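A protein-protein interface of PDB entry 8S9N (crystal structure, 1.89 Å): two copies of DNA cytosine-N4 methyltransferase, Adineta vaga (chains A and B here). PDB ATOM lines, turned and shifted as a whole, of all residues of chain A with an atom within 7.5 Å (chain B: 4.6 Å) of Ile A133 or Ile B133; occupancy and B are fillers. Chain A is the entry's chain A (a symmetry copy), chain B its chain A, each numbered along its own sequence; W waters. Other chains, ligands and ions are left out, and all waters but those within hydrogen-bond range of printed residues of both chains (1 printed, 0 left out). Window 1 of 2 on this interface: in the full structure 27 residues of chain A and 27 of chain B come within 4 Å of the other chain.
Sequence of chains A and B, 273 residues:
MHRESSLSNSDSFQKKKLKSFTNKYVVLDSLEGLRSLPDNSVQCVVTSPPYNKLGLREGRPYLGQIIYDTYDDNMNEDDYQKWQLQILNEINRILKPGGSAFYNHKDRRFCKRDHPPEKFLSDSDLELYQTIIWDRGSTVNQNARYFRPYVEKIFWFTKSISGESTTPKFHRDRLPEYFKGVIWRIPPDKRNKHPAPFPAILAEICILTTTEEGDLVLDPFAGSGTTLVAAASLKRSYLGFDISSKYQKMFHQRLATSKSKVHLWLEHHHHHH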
ATOM      1  N   GLN A 130     -18.413 -18.893   6.524  1.00  0.00           N
ATOM      2  CA  GLN A 130     -17.055 -19.410   6.425  1.00  0.00           C
ATOM      3  C   GLN A 130     -16.756 -20.190   7.695  1.00  0.00           C
ATOM      4  O   GLN A 130     -17.324 -19.910   8.754  1.00  0.00           O
ATOM      5  CB  GLN A 130     -16.032 -18.279   6.229  1.00  0.00           C
ATOM      6  CG  GLN A 130     -14.630 -18.734   5.833  1.00  0.00           C
ATOM      7  CD  GLN A 130     -13.690 -17.568   5.522  1.00  0.00           C
ATOM      8  OE1 GLN A 130     -13.844 -16.471   6.057  1.00  0.00           O
ATOM      9  NE2 GLN A 130     -12.717 -17.808   4.647  1.00  0.00           N
ATOM     10  N   THR A 131     -15.874 -21.179   7.577  1.00  0.00           N
ATOM     11  CA  THR A 131     -15.363 -21.900   8.734  1.00  0.00           C
ATOM     12  C   THR A 131     -13.947 -21.415   9.018  1.00  0.00           C
ATOM     13  O   THR A 131     -13.046 -21.599   8.197  1.00  0.00           O
ATOM     14  CB  THR A 131     -15.373 -23.411   8.508  1.00  0.00           C
ATOM     15  OG1 THR A 131     -16.713 -23.843   8.234  1.00  0.00           O
ATOM     16  CG2 THR A 131     -14.861 -24.126   9.756  1.00  0.00           C
ATOM     17  N   ILE A 132     -13.760 -20.799  10.167  1.00  0.00           N
ATOM     18  CA  ILE A 132     -12.454 -20.314  10.589  1.00  0.00           C
ATOM     19  C   ILE A 132     -11.767 -21.406  11.399  1.00  0.00           C
ATOM     20  O   ILE A 132     -12.419 -22.136  12.153  1.00  0.00           O
ATOM     21  CB  ILE A 132     -12.607 -19.011  11.392  1.00  0.00           C
ATOM     22  CG1 ILE A 132     -13.084 -17.887  10.462  1.00  0.00           C
ATOM     23  CG2 ILE A 132     -11.306 -18.642  12.110  1.00  0.00           C
ATOM     24  CD1 ILE A 132     -13.851 -16.788  11.191  1.00  0.00           C
ATOM     25  N   ILE A 133     -10.456 -21.542  11.218  1.00  0.00           N
ATOM     26  CA  ILE A 133      -9.659 -22.558  11.896  1.00  0.00           C
ATOM     27  C   ILE A 133      -8.898 -21.877  13.027  1.00  0.00           C
ATOM     28  O   ILE A 133      -8.011 -21.054  12.782  1.00  0.00           O
ATOM     29  CB  ILE A 133      -8.692 -23.259  10.931  1.00  0.00           C
ATOM     30  CG1 ILE A 133      -9.454 -23.928   9.784  1.00  0.00           C
ATOM     31  CG2 ILE A 133      -7.833 -24.271  11.676  1.00  0.00           C
ATOM     32  CD1 ILE A 133     -10.410 -25.008  10.230  1.00  0.00           C
ATOM     33  N   TRP A 134      -9.227 -22.221  14.268  1.00  0.00           N
ATOM     34  CA  TRP A 134      -8.510 -21.701  15.429  1.00  0.00           C
ATOM     35  C   TRP A 134      -7.393 -22.681  15.768  1.00  0.00           C
ATOM     36  O   TRP A 134      -7.648 -23.788  16.252  1.00  0.00           O
ATOM     37  CB  TRP A 134      -9.461 -21.483  16.606  1.00  0.00           C
ATOM     38  CG  TRP A 134      -8.787 -21.152  17.923  1.00  0.00           C
ATOM     39  CD1 TRP A 134      -7.515 -20.680  18.116  1.00  0.00           C
ATOM     40  CD2 TRP A 134      -9.364 -21.285  19.230  1.00  0.00           C
ATOM     41  NE1 TRP A 134      -7.271 -20.514  19.461  1.00  0.00           N
ATOM     42  CE2 TRP A 134      -8.386 -20.883  20.163  1.00  0.00           C
ATOM     43  CE3 TRP A 134     -10.610 -21.712  19.700  1.00  0.00           C
ATOM     44  CZ2 TRP A 134      -8.618 -20.892  21.541  1.00  0.00           C
ATOM     45  CZ3 TRP A 134     -10.839 -21.719  21.071  1.00  0.00           C
ATOM     46  CH2 TRP A 134      -9.847 -21.312  21.972  1.00  0.00           C
ATOM     47  N   ASP A 135      -6.156 -22.270  15.506  1.00  0.00           N
ATOM     48  CA  ASP A 135      -4.974 -23.097  15.726  1.00  0.00           C
ATOM     49  C   ASP A 135      -4.424 -22.768  17.111  1.00  0.00           C
ATOM     50  O   ASP A 135      -3.818 -21.710  17.308  1.00  0.00           O
ATOM     51  CB  ASP A 135      -3.949 -22.830  14.624  1.00  0.00           C
ATOM     52  CG  ASP A 135      -2.617 -23.530  14.853  1.00  0.00           C
ATOM     53  OD1 ASP A 135      -2.492 -24.346  15.790  1.00  0.00           O
ATOM     54  OD2 ASP A 135      -1.679 -23.255  14.075  1.00  0.00           O
ATOM     55  N   ARG A 136      -4.635 -23.671  18.070  1.00  0.00           N
ATOM     56  CA  ARG A 136      -4.238 -23.410  19.449  1.00  0.00           C
ATOM     57  C   ARG A 136      -2.751 -23.645  19.692  1.00  0.00           C
ATOM     58  O   ARG A 136      -2.273 -23.385  20.804  1.00  0.00           O
ATOM     59  CB  ARG A 136      -5.065 -24.268  20.414  1.00  0.00           C
ATOM     60  CG  ARG A 136      -6.571 -24.042  20.325  1.00  0.00           C
ATOM     61  CD  ARG A 136      -7.344 -24.838  21.382  1.00  0.00           C
ATOM     62  NE  ARG A 136      -7.376 -24.154  22.670  1.00  0.00           N
ATOM     63  CZ  ARG A 136      -8.337 -24.298  23.573  1.00  0.00           C
ATOM     64  NH1 ARG A 136      -9.371 -25.095  23.362  1.00  0.00           N
ATOM     65  NH2 ARG A 136      -8.264 -23.617  24.713  1.00  0.00           N
ATOM     66  N   TYR A 150      -4.925 -30.034  17.772  1.00  0.00           N
ATOM     67  CA  TYR A 150      -4.818 -28.726  18.402  1.00  0.00           C
ATOM     68  C   TYR A 150      -5.640 -27.661  17.679  1.00  0.00           C
ATOM     69  O   TYR A 150      -5.349 -26.468  17.810  1.00  0.00           O
ATOM     70  CB  TYR A 150      -3.350 -28.308  18.503  1.00  0.00           C
ATOM     71  CG  TYR A 150      -2.587 -28.407  17.207  1.00  0.00           C
ATOM     72  CD1 TYR A 150      -2.890 -27.573  16.139  1.00  0.00           C
ATOM     73  CD2 TYR A 150      -1.548 -29.317  17.055  1.00  0.00           C
ATOM     74  CE1 TYR A 150      -2.196 -27.652  14.952  1.00  0.00           C
ATOM     75  CE2 TYR A 150      -0.841 -29.399  15.869  1.00  0.00           C
ATOM     76  CZ  TYR A 150      -1.173 -28.567  14.820  1.00  0.00           C
ATOM     77  OH  TYR A 150      -0.483 -28.637  13.628  1.00  0.00           O
ATOM     78  N   VAL A 151      -6.671 -28.068  16.937  1.00  0.00           N
ATOM     79  CA  VAL A 151      -7.511 -27.167  16.154  1.00  0.00           C
ATOM     80  C   VAL A 151      -8.941 -27.213  16.677  1.00  0.00           C
ATOM     81  O   VAL A 151      -9.472 -28.292  16.960  1.00  0.00           O
ATOM     82  CB  VAL A 151      -7.478 -27.537  14.654  1.00  0.00           C
ATOM     83  CG1 VAL A 151      -8.758 -27.102  13.955  1.00  0.00           C
ATOM     84  CG2 VAL A 151      -6.275 -26.910  13.992  1.00  0.00           C
ATOM     85  N   GLU A 152      -9.562 -26.039  16.796  1.00  0.00           N
ATOM     86  CA  GLU A 152     -11.001 -25.916  16.965  1.00  0.00           C
ATOM     87  C   GLU A 152     -11.568 -25.084  15.819  1.00  0.00           C
ATOM     88  O   GLU A 152     -10.868 -24.275  15.214  1.00  0.00           O
ATOM     89  CB  GLU A 152     -11.359 -25.274  18.315  1.00  0.00           C
ATOM     90  CG  GLU A 152     -10.883 -26.088  19.510  1.00  0.00           C
ATOM     91  CD  GLU A 152     -11.412 -25.566  20.834  1.00  0.00           C
ATOM     92  OE1 GLU A 152     -12.326 -24.714  20.831  1.00  0.00           O
ATOM     93  OE2 GLU A 152     -10.911 -26.016  21.883  1.00  0.00           O
ATOM     94  N   LYS A 153     -12.846 -25.299  15.521  1.00  0.00           N
ATOM     95  CA  LYS A 153     -13.546 -24.566  14.474  1.00  0.00           C
ATOM     96  C   LYS A 153     -14.315 -23.387  15.061  1.00  0.00           C
ATOM     97  O   LYS A 153     -14.870 -23.475  16.161  1.00  0.00           O
ATOM     98  CB  LYS A 153     -14.520 -25.478  13.724  1.00  0.00           C
ATOM     99  CG  LYS A 153     -13.867 -26.564  12.891  1.00  0.00           C
ATOM    100  CD  LYS A 153     -14.886 -27.644  12.548  1.00  0.00           C
ATOM    101  CE  LYS A 153     -14.350 -28.628  11.523  1.00  0.00           C
ATOM    102  NZ  LYS A 153     -15.303 -29.759  11.318  1.00  0.00           N
ATOM    103  N   ILE A 154     -14.341 -22.286  14.319  1.00  0.00           N
ATOM    104  CA  ILE A 154     -15.194 -21.139  14.607  1.00  0.00           C
ATOM    105  C   ILE A 154     -16.099 -20.962  13.398  1.00  0.00           C
ATOM    106  O   ILE A 154     -15.641 -20.526  12.334  1.00  0.00           O
ATOM    107  CB  ILE A 154     -14.383 -19.864  14.875  1.00  0.00           C
ATOM    108  CG1 ILE A 154     -13.440 -20.067  16.061  1.00  0.00           C
ATOM    109  CG2 ILE A 154     -15.313 -18.671  15.118  1.00  0.00           C
ATOM    110  CD1 ILE A 154     -12.382 -18.993  16.166  1.00  0.00           C
ATOM    111  N   PHE A 155     -17.373 -21.307  13.545  1.00  0.00           N
ATOM    112  CA  PHE A 155     -18.304 -21.201  12.429  1.00  0.00           C
ATOM    113  C   PHE A 155     -18.839 -19.776  12.336  1.00  0.00           C
ATOM    114  O   PHE A 155     -19.453 -19.268  13.282  1.00  0.00           O
ATOM    115  CB  PHE A 155     -19.437 -22.210  12.587  1.00  0.00           C
ATOM    116  CG  PHE A 155     -18.972 -23.644  12.552  1.00  0.00           C
ATOM    117  CD1 PHE A 155     -18.690 -24.267  11.343  1.00  0.00           C
ATOM    118  CD2 PHE A 155     -18.804 -24.362  13.726  1.00  0.00           C
ATOM    119  CE1 PHE A 155     -18.258 -25.583  11.309  1.00  0.00           C
ATOM    120  CE2 PHE A 155     -18.373 -25.679  13.697  1.00  0.00           C
ATOM    121  CZ  PHE A 155     -18.102 -26.289  12.489  1.00  0.00           C
ATOM    122  N   GLY A 181      -6.074 -14.143   7.662  1.00  0.00           N
ATOM    123  CA  GLY A 181      -6.269 -15.429   7.028  1.00  0.00           C
ATOM    124  C   GLY A 181      -7.278 -16.297   7.768  1.00  0.00           C
ATOM    125  O   GLY A 181      -7.703 -16.003   8.881  1.00  0.00           O
ATOM    126  N   VAL A 182      -7.653 -17.403   7.122  1.00  0.00           N
ATOM    127  CA  VAL A 182      -8.683 -18.275   7.678  1.00  0.00           C
ATOM    128  C   VAL A 182      -8.181 -19.119   8.848  1.00  0.00           C
ATOM    129  O   VAL A 182      -8.991 -19.736   9.554  1.00  0.00           O
ATOM    130  CB  VAL A 182      -9.268 -19.135   6.537  1.00  0.00           C
ATOM    131  CG1 VAL A 182      -8.263 -20.174   6.067  1.00  0.00           C
ATOM    132  CG2 VAL A 182     -10.592 -19.780   6.952  1.00  0.00           C
ATOM    133  N   ILE A 183      -6.873 -19.149   9.102  1.00  0.00           N
ATOM    134  CA  ILE A 183      -6.313 -19.796  10.287  1.00  0.00           C
ATOM    135  C   ILE A 183      -5.845 -18.712  11.244  1.00  0.00           C
ATOM    136  O   ILE A 183      -5.048 -17.844  10.864  1.00  0.00           O
ATOM    137  CB  ILE A 183      -5.144 -20.735   9.943  1.00  0.00           C
ATOM    138  CG1 ILE A 183      -5.578 -21.848   8.992  1.00  0.00           C
ATOM    139  CG2 ILE A 183      -4.570 -21.353  11.214  1.00  0.00           C
ATOM    140  CD1 ILE A 183      -4.482 -22.863   8.745  1.00  0.00           C
ATOM    141  N   TRP A 184      -6.330 -18.763  12.484  1.00  0.00           N
ATOM    142  CA  TRP A 184      -5.880 -17.877  13.552  1.00  0.00           C
ATOM    143  C   TRP A 184      -5.020 -18.679  14.517  1.00  0.00           C
ATOM    144  O   TRP A 184      -5.510 -19.630  15.137  1.00  0.00           O
ATOM    145  CB  TRP A 184      -7.056 -17.264  14.311  1.00  0.00           C
ATOM    146  CG  TRP A 184      -8.034 -16.512  13.471  1.00  0.00           C
ATOM    147  CD1 TRP A 184      -7.862 -16.071  12.187  1.00  0.00           C
ATOM    148  CD2 TRP A 184      -9.350 -16.112  13.862  1.00  0.00           C
ATOM    149  NE1 TRP A 184      -8.997 -15.424  11.755  1.00  0.00           N
ATOM    150  CE2 TRP A 184      -9.923 -15.429  12.767  1.00  0.00           C
ATOM    151  CE3 TRP A 184     -10.099 -16.258  15.038  1.00  0.00           C
ATOM    152  CZ2 TRP A 184     -11.214 -14.901  12.808  1.00  0.00           C
ATOM    153  CZ3 TRP A 184     -11.381 -15.729  15.079  1.00  0.00           C
ATOM    154  CH2 TRP A 184     -11.926 -15.059  13.967  1.00  0.00           C
ATOM    155  N   ARG A 185      -3.753 -18.291  14.657  1.00  0.00           N
ATOM    156  CA  ARG A 185      -2.840 -18.941  15.599  1.00  0.00           C
ATOM    157  C   ARG A 185      -2.901 -18.184  16.921  1.00  0.00           C
ATOM    158  O   ARG A 185      -2.275 -17.133  17.080  1.00  0.00           O
ATOM    159  CB  ARG A 185      -1.422 -18.981  15.040  1.00  0.00           C
ATOM    160  N   ILE A 186      -3.659 -18.720  17.873  1.00  0.00           N
ATOM    161  CA  ILE A 186      -3.914 -18.061  19.152  1.00  0.00           C
ATOM    162  C   ILE A 186      -3.737 -19.069  20.282  1.00  0.00           C
ATOM    163  O   ILE A 186      -4.537 -20.009  20.394  1.00  0.00           O
ATOM    164  CB  ILE A 186      -5.325 -17.449  19.191  1.00  0.00           C
ATOM    165  CG1 ILE A 186      -5.542 -16.494  18.019  1.00  0.00           C
ATOM    166  CG2 ILE A 186      -5.549 -16.729  20.501  1.00  0.00           C
ATOM    167  CD1 ILE A 186      -6.924 -15.874  17.984  1.00  0.00           C
ATOM    168  N   THR B 131     -10.500 -34.863  10.356  1.00  0.00           N
ATOM    169  CA  THR B 131     -10.380 -33.874   9.293  1.00  0.00           C
ATOM    170  C   THR B 131      -9.027 -33.188   9.421  1.00  0.00           C
ATOM    171  O   THR B 131      -8.761 -32.510  10.416  1.00  0.00           O
ATOM    172  CB  THR B 131     -11.508 -32.845   9.350  1.00  0.00           C
ATOM    173  OG1 THR B 131     -12.771 -33.514   9.236  1.00  0.00           O
ATOM    174  CG2 THR B 131     -11.362 -31.851   8.200  1.00  0.00           C
ATOM    175  N   ILE B 132      -8.184 -33.368   8.426  1.00  0.00           N
ATOM    176  CA  ILE B 132      -6.869 -32.744   8.393  1.00  0.00           C
ATOM    177  C   ILE B 132      -6.981 -31.409   7.670  1.00  0.00           C
ATOM    178  O   ILE B 132      -7.741 -31.276   6.705  1.00  0.00           O
ATOM    179  CB  ILE B 132      -5.853 -33.682   7.719  1.00  0.00           C
ATOM    180  CG1 ILE B 132      -5.610 -34.905   8.615  1.00  0.00           C
ATOM    181  CG2 ILE B 132      -4.551 -32.950   7.389  1.00  0.00           C
ATOM    182  CD1 ILE B 132      -5.165 -36.140   7.837  1.00  0.00           C
ATOM    183  N   ILE B 133      -6.249 -30.409   8.155  1.00  0.00           N
ATOM    184  CA  ILE B 133      -6.266 -29.063   7.593  1.00  0.00           C
ATOM    185  C   ILE B 133      -5.000 -28.886   6.764  1.00  0.00           C
ATOM    186  O   ILE B 133      -3.891 -28.865   7.306  1.00  0.00           O
ATOM    187  CB  ILE B 133      -6.356 -27.991   8.688  1.00  0.00           C
ATOM    188  CG1 ILE B 133      -7.619 -28.178   9.534  1.00  0.00           C
ATOM    189  CG2 ILE B 133      -6.313 -26.597   8.078  1.00  0.00           C
ATOM    190  CD1 ILE B 133      -8.905 -28.047   8.754  1.00  0.00           C
ATOM    191  N   TRP B 134      -5.154 -28.747   5.450  1.00  0.00           N
ATOM    192  CA  TRP B 134      -4.022 -28.485   4.565  1.00  0.00           C
ATOM    193  C   TRP B 134      -3.886 -26.974   4.413  1.00  0.00           C
ATOM    194  O   TRP B 134      -4.715 -26.326   3.767  1.00  0.00           O
ATOM    195  CB  TRP B 134      -4.210 -29.185   3.219  1.00  0.00           C
ATOM    196  CG  TRP B 134      -3.202 -28.804   2.152  1.00  0.00           C
ATOM    197  CD1 TRP B 134      -1.975 -28.219   2.331  1.00  0.00           C
ATOM    198  CD2 TRP B 134      -3.355 -28.979   0.736  1.00  0.00           C
ATOM    199  NE1 TRP B 134      -1.362 -28.023   1.114  1.00  0.00           N
ATOM    200  CE2 TRP B 134      -2.190 -28.475   0.122  1.00  0.00           C
ATOM    201  CE3 TRP B 134      -4.368 -29.508  -0.070  1.00  0.00           C
ATOM    202  CZ2 TRP B 134      -2.009 -28.488  -1.263  1.00  0.00           C
ATOM    203  CZ3 TRP B 134      -4.186 -29.521  -1.448  1.00  0.00           C
ATOM    204  CH2 TRP B 134      -3.015 -29.014  -2.027  1.00  0.00           C
ATOM    205  N   ASP B 135      -2.838 -26.419   5.015  1.00  0.00           N
ATOM    206  CA  ASP B 135      -2.580 -24.983   5.009  1.00  0.00           C
ATOM    207  C   ASP B 135      -1.639 -24.682   3.847  1.00  0.00           C
ATOM    208  O   ASP B 135      -0.442 -24.977   3.918  1.00  0.00           O
ATOM    209  CB  ASP B 135      -1.984 -24.564   6.353  1.00  0.00           C
ATOM    210  CG  ASP B 135      -1.534 -23.110   6.390  1.00  0.00           C
ATOM    211  OD1 ASP B 135      -1.794 -22.352   5.433  1.00  0.00           O
ATOM    212  OD2 ASP B 135      -0.910 -22.724   7.400  1.00  0.00           O
ATOM    213  N   VAL B 151      -6.911 -22.561   2.901  1.00  0.00           N
ATOM    214  CA  VAL B 151      -7.029 -23.868   3.542  1.00  0.00           C
ATOM    215  C   VAL B 151      -7.882 -24.788   2.679  1.00  0.00           C
ATOM    216  O   VAL B 151      -8.925 -24.375   2.161  1.00  0.00           O
ATOM    217  CB  VAL B 151      -7.639 -23.742   4.955  1.00  0.00           C
ATOM    218  CG1 VAL B 151      -8.357 -25.023   5.357  1.00  0.00           C
ATOM    219  CG2 VAL B 151      -6.562 -23.405   5.957  1.00  0.00           C
ATOM    220  N   GLU B 152      -7.438 -26.037   2.533  1.00  0.00           N
ATOM    221  CA  GLU B 152      -8.267 -27.119   2.026  1.00  0.00           C
ATOM    222  C   GLU B 152      -8.342 -28.223   3.076  1.00  0.00           C
ATOM    223  O   GLU B 152      -7.457 -28.361   3.917  1.00  0.00           O
ATOM    224  CB  GLU B 152      -7.719 -27.681   0.704  1.00  0.00           C
ATOM    225  CG  GLU B 152      -7.679 -26.649  -0.413  1.00  0.00           C
ATOM    226  CD  GLU B 152      -7.334 -27.249  -1.766  1.00  0.00           C
ATOM    227  OE1 GLU B 152      -7.343 -28.491  -1.900  1.00  0.00           O
ATOM    228  OE2 GLU B 152      -7.058 -26.470  -2.698  1.00  0.00           O
ATOM    229  N   VAL B 182      -2.485 -31.770  13.229  1.00  0.00           N
ATOM    230  CA  VAL B 182      -3.647 -31.825  12.346  1.00  0.00           C
ATOM    231  C   VAL B 182      -3.617 -30.756  11.256  1.00  0.00           C
ATOM    232  O   VAL B 182      -4.415 -30.820  10.310  1.00  0.00           O
ATOM    233  CB  VAL B 182      -4.925 -31.753  13.210  1.00  0.00           C
ATOM    234  CG1 VAL B 182      -5.104 -30.365  13.803  1.00  0.00           C
ATOM    235  CG2 VAL B 182      -6.156 -32.189  12.415  1.00  0.00           C
ATOM    236  N   ILE B 183      -2.705 -29.787  11.332  1.00  0.00           N
ATOM    237  CA  ILE B 183      -2.495 -28.814  10.262  1.00  0.00           C
ATOM    238  C   ILE B 183      -1.182 -29.145   9.570  1.00  0.00           C
ATOM    239  O   ILE B 183      -0.136 -29.233  10.225  1.00  0.00           O
ATOM    240  CB  ILE B 183      -2.464 -27.367  10.784  1.00  0.00           C
ATOM    241  CG1 ILE B 183      -3.772 -26.992  11.476  1.00  0.00           C
ATOM    242  CG2 ILE B 183      -2.202 -26.396   9.638  1.00  0.00           C
ATOM    243  CD1 ILE B 183      -3.820 -25.533  11.879  1.00  0.00           C
ATOM    244  N   TRP B 184      -1.233 -29.321   8.250  1.00  0.00           N
ATOM    245  CA  TRP B 184      -0.045 -29.513   7.426  1.00  0.00           C
ATOM    246  C   TRP B 184       0.201 -28.243   6.625  1.00  0.00           C
ATOM    247  O   TRP B 184      -0.641 -27.857   5.807  1.00  0.00           O
ATOM    248  CB  TRP B 184      -0.207 -30.693   6.468  1.00  0.00           C
ATOM    249  CG  TRP B 184      -0.537 -31.997   7.113  1.00  0.00           C
ATOM    250  CD1 TRP B 184      -0.430 -32.321   8.439  1.00  0.00           C
ATOM    251  CD2 TRP B 184      -1.033 -33.164   6.452  1.00  0.00           C
ATOM    252  NE1 TRP B 184      -0.836 -33.621   8.641  1.00  0.00           N
ATOM    253  CE2 TRP B 184      -1.205 -34.162   7.436  1.00  0.00           C
ATOM    254  CE3 TRP B 184      -1.342 -33.467   5.118  1.00  0.00           C
ATOM    255  CZ2 TRP B 184      -1.681 -35.438   7.132  1.00  0.00           C
ATOM    256  CZ3 TRP B 184      -1.812 -34.736   4.817  1.00  0.00           C
ATOM    257  CH2 TRP B 184      -1.979 -35.707   5.823  1.00  0.00           C
HETATM  258  O   HOH W   1     -14.567 -31.273   9.148  1.00  0.00           O
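The backbone NH of Ile B183 sits at hydrogen-bond distance from the side-chain hydroxyl of Tyr A150 (3.4 Å).
The backbone NH (N) of Ile A133 lies within hydrogen-bond range of the backbone carbonyl oxygen (O) of Val A182, 2.9 Å away. N of Arg A136 lies within hydrogen-bond range of O of Tyr A150 (2.9 Å). The backbone carbonyl oxygen (O) of Asp A135 lies within hydrogen-bond range of the backbone NH (N) of Ile A186 (3.0 Å). The backbone NH (N) of Asp A135 is in hydrogen-bond range of the backbone carbonyl oxygen (O) of Trp A184, 2.7 Å away. N of Asp B135 is in hydrogen-bond range of O of Trp B184 (2.7 Å). The backbone carbonyl oxygen (O) of Ile B133 lies within hydrogen-bond range of the backbone NH (N) of Trp B184, at 2.9 Å.
Among the printed residues, pairs that only touch across the chains: Val A151 with Ile B183, Ile A183 with Val B151, Val A151 with Val B182, Val A182 with Val B151, Ile A133 with Ile B133, Tyr A150 with Val B182, Ile A183 with Asp B135 and Asp A135 with Ile B183.
Printed residues of chain A within 4 Å of Ile B133: Ile A133. Of the printed residues of chain B, Ile A183 touches Asp B135 and Val B151. Printed residues of chain B within 4 Å of Val A182: Val B151 (3.7 Å). Thr A131 touches none of the printed residues of chain B. The nearest printed residue of chain B that does not touch Asp A135 is Asp B135 (6.7 Å).
Printed residues of chain B that touch a printed residue of chain A: Ile B133, Asp B135, Val B151, Val B182 and Ile B183. Printed residues of chain A that touch a printed residue of chain B: Ile A133, Asp A135, Tyr A150, Val A151, Val A182 and Ile A183. Along chain A the printed residues that touch a printed residue of chain B span positions 133 to 183. Among the printed residues, 9 pairs touch across the chains.
Ile B133 touches its own counterpart, Ile A133. Asp A135 touches Ile B183, and with the chains exchanged Ile A183 touches Asp B135. Val A151 touches Val B182, and with the chains exchanged Val A182 touches Val B151. Val A151 touches Ile B183, and with the chains exchanged Ile A183 touches Val B151. 10 positions are printed for both chains.
Water W1 bridges NZ of Lys A153 (2.7 Å) and OG1 of Thr B131 (2.9 Å).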
